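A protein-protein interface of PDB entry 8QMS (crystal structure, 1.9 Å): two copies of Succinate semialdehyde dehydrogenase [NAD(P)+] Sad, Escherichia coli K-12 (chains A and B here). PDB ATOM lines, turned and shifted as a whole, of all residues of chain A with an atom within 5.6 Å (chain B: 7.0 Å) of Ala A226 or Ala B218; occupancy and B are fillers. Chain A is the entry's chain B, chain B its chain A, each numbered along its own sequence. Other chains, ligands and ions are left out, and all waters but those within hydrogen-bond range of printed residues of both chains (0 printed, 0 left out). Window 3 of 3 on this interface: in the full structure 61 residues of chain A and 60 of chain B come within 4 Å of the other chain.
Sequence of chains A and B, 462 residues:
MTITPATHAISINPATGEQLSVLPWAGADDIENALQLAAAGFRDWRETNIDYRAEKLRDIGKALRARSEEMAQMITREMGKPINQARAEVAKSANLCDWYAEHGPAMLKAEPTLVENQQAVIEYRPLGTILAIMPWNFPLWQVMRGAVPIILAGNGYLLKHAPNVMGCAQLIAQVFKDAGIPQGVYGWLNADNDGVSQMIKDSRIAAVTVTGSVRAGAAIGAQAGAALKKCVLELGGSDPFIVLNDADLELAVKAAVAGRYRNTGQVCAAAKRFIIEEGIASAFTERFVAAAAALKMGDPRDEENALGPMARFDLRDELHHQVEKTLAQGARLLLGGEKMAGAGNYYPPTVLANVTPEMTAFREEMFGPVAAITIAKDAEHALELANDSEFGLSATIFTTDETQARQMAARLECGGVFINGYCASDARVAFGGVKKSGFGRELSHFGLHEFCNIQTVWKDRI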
ATOM      1  N   GLY A 221       7.050   8.689 -25.862  1.00  0.00           N
ATOM      2  CA  GLY A 221       8.322   8.679 -26.570  1.00  0.00           C
ATOM      3  C   GLY A 221       9.428   9.375 -25.801  1.00  0.00           C
ATOM      4  O   GLY A 221      10.576   8.918 -25.794  1.00  0.00           O
ATOM      5  N   ALA A 222       9.100  10.489 -25.139  1.00  0.00           N
ATOM      6  CA  ALA A 222      10.089  11.175 -24.313  1.00  0.00           C
ATOM      7  C   ALA A 222      10.590  10.276 -23.187  1.00  0.00           C
ATOM      8  O   ALA A 222      11.786  10.275 -22.868  1.00  0.00           O
ATOM      9  CB  ALA A 222       9.498  12.465 -23.744  1.00  0.00           C
ATOM     10  N   GLN A 223       9.690   9.505 -22.572  1.00  0.00           N
ATOM     11  CA  GLN A 223      10.093   8.641 -21.467  1.00  0.00           C
ATOM     12  C   GLN A 223      10.925   7.467 -21.957  1.00  0.00           C
ATOM     13  O   GLN A 223      11.897   7.068 -21.303  1.00  0.00           O
ATOM     14  CB  GLN A 223       8.863   8.133 -20.715  1.00  0.00           C
ATOM     15  CG  GLN A 223       8.028   9.216 -20.070  1.00  0.00           C
ATOM     16  CD  GLN A 223       6.816   8.639 -19.365  1.00  0.00           C
ATOM     17  OE1 GLN A 223       6.950   7.908 -18.383  1.00  0.00           O
ATOM     18  NE2 GLN A 223       5.632   8.941 -19.875  1.00  0.00           N
ATOM     19  N   ALA A 224      10.544   6.880 -23.094  1.00  0.00           N
ATOM     20  CA  ALA A 224      11.324   5.778 -23.645  1.00  0.00           C
ATOM     21  C   ALA A 224      12.750   6.222 -23.943  1.00  0.00           C
ATOM     22  O   ALA A 224      13.714   5.527 -23.605  1.00  0.00           O
ATOM     23  CB  ALA A 224      10.643   5.228 -24.900  1.00  0.00           C
ATOM     24  N   GLY A 225      12.904   7.393 -24.566  1.00  0.00           N
ATOM     25  CA  GLY A 225      14.240   7.900 -24.839  1.00  0.00           C
ATOM     26  C   GLY A 225      15.034   8.154 -23.571  1.00  0.00           C
ATOM     27  O   GLY A 225      16.212   7.786 -23.471  1.00  0.00           O
ATOM     28  N   ALA A 226      14.396   8.773 -22.574  1.00  0.00           N
ATOM     29  CA  ALA A 226      15.080   9.024 -21.308  1.00  0.00           C
ATOM     30  C   ALA A 226      15.513   7.729 -20.634  1.00  0.00           C
ATOM     31  O   ALA A 226      16.534   7.707 -19.937  1.00  0.00           O
ATOM     32  CB  ALA A 226      14.180   9.834 -20.376  1.00  0.00           C
ATOM     33  N   ALA A 227      14.760   6.647 -20.831  1.00  0.00           N
ATOM     34  CA  ALA A 227      15.117   5.332 -20.313  1.00  0.00           C
ATOM     35  C   ALA A 227      15.976   4.522 -21.281  1.00  0.00           C
ATOM     36  O   ALA A 227      16.293   3.363 -20.988  1.00  0.00           O
ATOM     37  CB  ALA A 227      13.849   4.544 -19.967  1.00  0.00           C
ATOM     38  N   LEU A 228      16.357   5.103 -22.420  1.00  0.00           N
ATOM     39  CA  LEU A 228      17.171   4.425 -23.430  1.00  0.00           C
ATOM     40  C   LEU A 228      16.481   3.165 -23.950  1.00  0.00           C
ATOM     41  O   LEU A 228      17.121   2.136 -24.179  1.00  0.00           O
ATOM     42  CB  LEU A 228      18.568   4.099 -22.894  1.00  0.00           C
ATOM     43  CG  LEU A 228      19.395   5.299 -22.447  1.00  0.00           C
ATOM     44  CD1 LEU A 228      20.742   4.826 -21.934  1.00  0.00           C
ATOM     45  CD2 LEU A 228      19.559   6.284 -23.598  1.00  0.00           C
ATOM     46  N   VAL B 210      22.776   9.775 -32.622  1.00  0.00           N
ATOM     47  CA  VAL B 210      23.698  10.128 -31.550  1.00  0.00           C
ATOM     48  C   VAL B 210      24.709   9.009 -31.376  1.00  0.00           C
ATOM     49  O   VAL B 210      24.338   7.834 -31.279  1.00  0.00           O
ATOM     50  CB  VAL B 210      22.974  10.388 -30.216  1.00  0.00           C
ATOM     51  CG1 VAL B 210      23.983  10.783 -29.135  1.00  0.00           C
ATOM     52  CG2 VAL B 210      21.907  11.456 -30.384  1.00  0.00           C
ATOM     53  N   SER B 213      28.049   9.066 -25.052  1.00  0.00           N
ATOM     54  CA  SER B 213      27.917   8.396 -23.771  1.00  0.00           C
ATOM     55  C   SER B 213      26.455   8.055 -23.483  1.00  0.00           C
ATOM     56  O   SER B 213      25.526   8.551 -24.131  1.00  0.00           O
ATOM     57  CB  SER B 213      28.477   9.263 -22.645  1.00  0.00           C
ATOM     58  OG  SER B 213      27.707  10.446 -22.494  1.00  0.00           O
ATOM     59  N   VAL B 214      26.268   7.188 -22.485  1.00  0.00           N
ATOM     60  CA  VAL B 214      24.927   6.850 -22.011  1.00  0.00           C
ATOM     61  C   VAL B 214      24.195   8.106 -21.565  1.00  0.00           C
ATOM     62  O   VAL B 214      23.011   8.300 -21.872  1.00  0.00           O
ATOM     63  CB  VAL B 214      25.014   5.812 -20.874  1.00  0.00           C
ATOM     64  CG1 VAL B 214      23.662   5.650 -20.190  1.00  0.00           C
ATOM     65  CG2 VAL B 214      25.503   4.481 -21.404  1.00  0.00           C
ATOM     66  N   ARG B 215      24.898   8.994 -20.857  1.00  0.00           N
ATOM     67  CA  ARG B 215      24.268  10.208 -20.349  1.00  0.00           C
ATOM     68  C   ARG B 215      23.792  11.106 -21.485  1.00  0.00           C
ATOM     69  O   ARG B 215      22.690  11.668 -21.425  1.00  0.00           O
ATOM     70  CB  ARG B 215      25.250  10.955 -19.448  1.00  0.00           C
ATOM     71  CG  ARG B 215      24.725  12.258 -18.865  1.00  0.00           C
ATOM     72  CD  ARG B 215      25.858  13.055 -18.210  1.00  0.00           C
ATOM     73  NE  ARG B 215      26.783  13.603 -19.197  1.00  0.00           N
ATOM     74  CZ  ARG B 215      27.933  13.044 -19.560  1.00  0.00           C
ATOM     75  NH1 ARG B 215      28.361  11.917 -19.012  1.00  0.00           N
ATOM     76  NH2 ARG B 215      28.670  13.631 -20.500  1.00  0.00           N
ATOM     77  N   ALA B 216      24.609  11.260 -22.528  1.00  0.00           N
ATOM     78  CA  ALA B 216      24.200  12.078 -23.665  1.00  0.00           C
ATOM     79  C   ALA B 216      23.024  11.450 -24.401  1.00  0.00           C
ATOM     80  O   ALA B 216      22.090  12.154 -24.805  1.00  0.00           O
ATOM     81  CB  ALA B 216      25.373  12.275 -24.620  1.00  0.00           C
ATOM     82  N   GLY B 217      23.062  10.130 -24.591  1.00  0.00           N
ATOM     83  CA  GLY B 217      21.976   9.457 -25.282  1.00  0.00           C
ATOM     84  C   GLY B 217      20.649   9.600 -24.567  1.00  0.00           C
ATOM     85  O   GLY B 217      19.610   9.786 -25.204  1.00  0.00           O
ATOM     86  N   ALA B 218      20.660   9.519 -23.233  1.00  0.00           N
ATOM     87  CA  ALA B 218      19.420   9.691 -22.484  1.00  0.00           C
ATOM     88  C   ALA B 218      18.930  11.130 -22.556  1.00  0.00           C
ATOM     89  O   ALA B 218      17.724  11.374 -22.695  1.00  0.00           O
ATOM     90  CB  ALA B 218      19.610   9.253 -21.033  1.00  0.00           C
ATOM     91  N   ALA B 219      19.850  12.094 -22.474  1.00  0.00           N
ATOM     92  CA  ALA B 219      19.479  13.503 -22.572  1.00  0.00           C
ATOM     93  C   ALA B 219      18.881  13.822 -23.939  1.00  0.00           C
ATOM     94  O   ALA B 219      17.814  14.437 -24.037  1.00  0.00           O
ATOM     95  CB  ALA B 219      20.703  14.385 -22.298  1.00  0.00           C
ATOM     96  N   ILE B 220      19.552  13.394 -25.006  1.00  0.00           N
ATOM     97  CA  ILE B 220      19.107  13.712 -26.357  1.00  0.00           C
ATOM     98  C   ILE B 220      17.933  12.832 -26.767  1.00  0.00           C
ATOM     99  O   ILE B 220      16.991  13.301 -27.420  1.00  0.00           O
ATOM    100  CB  ILE B 220      20.283  13.578 -27.337  1.00  0.00           C
ATOM    101  CG1 ILE B 220      21.414  14.533 -26.937  1.00  0.00           C
ATOM    102  CG2 ILE B 220      19.816  13.853 -28.757  1.00  0.00           C
ATOM    103  CD1 ILE B 220      22.714  14.295 -27.682  1.00  0.00           C
ATOM    104  N   GLY B 221      17.970  11.546 -26.399  1.00  0.00           N
ATOM    105  CA  GLY B 221      16.885  10.649 -26.765  1.00  0.00           C
ATOM    106  C   GLY B 221      15.547  11.089 -26.207  1.00  0.00           C
ATOM    107  O   GLY B 221      14.519  10.998 -26.883  1.00  0.00           O
ATOM    108  N   ALA B 222      15.539  11.573 -24.964  1.00  0.00           N
ATOM    109  CA  ALA B 222      14.303  12.084 -24.379  1.00  0.00           C
ATOM    110  C   ALA B 222      13.757  13.256 -25.185  1.00  0.00           C
ATOM    111  O   ALA B 222      12.540  13.381 -25.377  1.00  0.00           O
ATOM    112  CB  ALA B 222      14.548  12.496 -22.929  1.00  0.00           C
ATOM    113  N   GLN B 223      14.647  14.126 -25.665  1.00  0.00           N
ATOM    114  CA  GLN B 223      14.211  15.284 -26.434  1.00  0.00           C
ATOM    115  C   GLN B 223      13.701  14.873 -27.807  1.00  0.00           C
ATOM    116  O   GLN B 223      12.724  15.445 -28.309  1.00  0.00           O
ATOM    117  CB  GLN B 223      15.360  16.285 -26.572  1.00  0.00           C
ATOM    118  CG  GLN B 223      15.873  16.833 -25.259  1.00  0.00           C
ATOM    119  CD  GLN B 223      16.987  17.836 -25.472  1.00  0.00           C
ATOM    120  OE1 GLN B 223      16.753  18.938 -25.966  1.00  0.00           O
ATOM    121  NE2 GLN B 223      18.206  17.455 -25.119  1.00  0.00           N
ATOM    122  N   LEU B 233      20.572   5.631 -31.234  1.00  0.00           N
ATOM    123  CA  LEU B 233      21.457   5.882 -30.103  1.00  0.00           C
ATOM    124  C   LEU B 233      22.534   4.808 -30.092  1.00  0.00           C
ATOM    125  O   LEU B 233      22.246   3.629 -29.859  1.00  0.00           O
ATOM    126  CB  LEU B 233      20.678   5.904 -28.786  1.00  0.00           C
ATOM    127  CG  LEU B 233      19.597   6.984 -28.654  1.00  0.00           C
ATOM    128  CD1 LEU B 233      18.972   6.957 -27.265  1.00  0.00           C
ATOM    129  CD2 LEU B 233      20.147   8.377 -28.965  1.00  0.00           C
ATOM    130  N   LEU B 235      25.620   4.196 -28.004  1.00  0.00           N
ATOM    131  CA  LEU B 235      26.141   4.746 -26.773  1.00  0.00           C
ATOM    132  C   LEU B 235      27.350   3.936 -26.287  1.00  0.00           C
ATOM    133  O   LEU B 235      28.036   3.276 -27.082  1.00  0.00           O
ATOM    134  CB  LEU B 235      25.008   4.825 -25.755  1.00  0.00           C
ATOM    135  CG  LEU B 235      23.765   5.516 -26.344  1.00  0.00           C
ATOM    136  CD1 LEU B 235      22.622   5.571 -25.351  1.00  0.00           C
ATOM    137  CD2 LEU B 235      24.112   6.920 -26.853  1.00  0.00           C
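Among the printed residues, pairs that only touch across the chains: Ala A222 with Ala B222, Gly A225 with Ala B218, Gly A225 with Gly B221, Gly A225 with Ala B222, Ala A226 with Ala B218, Ala A226 with Ala B222, Leu A228 with Val B214, Leu A228 with Gly B217, Leu A228 with Ala B218, Leu A228 with Leu B233 and Leu A228 with Leu B235.
Ala A226 touches just these residues of chain B: Ala B218 and Ala B222.
Ala B218 touches just these residues of chain A: Gly A225 (3.9 Å), Ala A226 (3.6 Å) and Leu A228 (3.4 Å).
Gly A225 touches just these residues of chain B: Ala B218 (3.9 Å), Gly B221 (3.7 Å) and Ala B222 (3.7 Å).
Printed residues of chain A within 4 Å of Leu B233: Leu A228.
Printed residues of chain A within 4 Å of Gly B217: Leu A228.
Printed residues of chain B within 4 Å of Ala A222: Ala B222 (3.4 Å).
Of the printed residues of chain A, Gly B221 touches Gly A225 (3.7 Å).
Of the printed residues of chain A, Ala B222 touches Ala A222, Gly A225 and Ala A226.
The nearest residue of chain B that does not touch Ala A226 is Gly B221 (4.5 Å).
The nearest residue of chain A that does not touch Ala B218 is Ala A227 (5.5 Å).
The nearest printed residue of chain B that does not touch Ala A222 is Gly B221 (4.9 Å).
Along chain A the printed residues that touch a printed residue of chain B span positions 222 to 228.
Hydrophobic or aromatic side chains of chain B that line the printed part of chain A: Val B214, Ala B218, Ala B222, Leu B233 and Leu B235.
Among the printed residues, no Asp or Glu carboxylate lies within 4 Å of a Lys or Arg side-chain nitrogen of the other chain.
Ala B222 touches its own counterpart, Ala A222.
Positions printed for both chains: 221, 222 and 223.
Of the 11 pairs that touch across the chains among the printed residues, 1 has its exchanged pair printed and touching as well.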
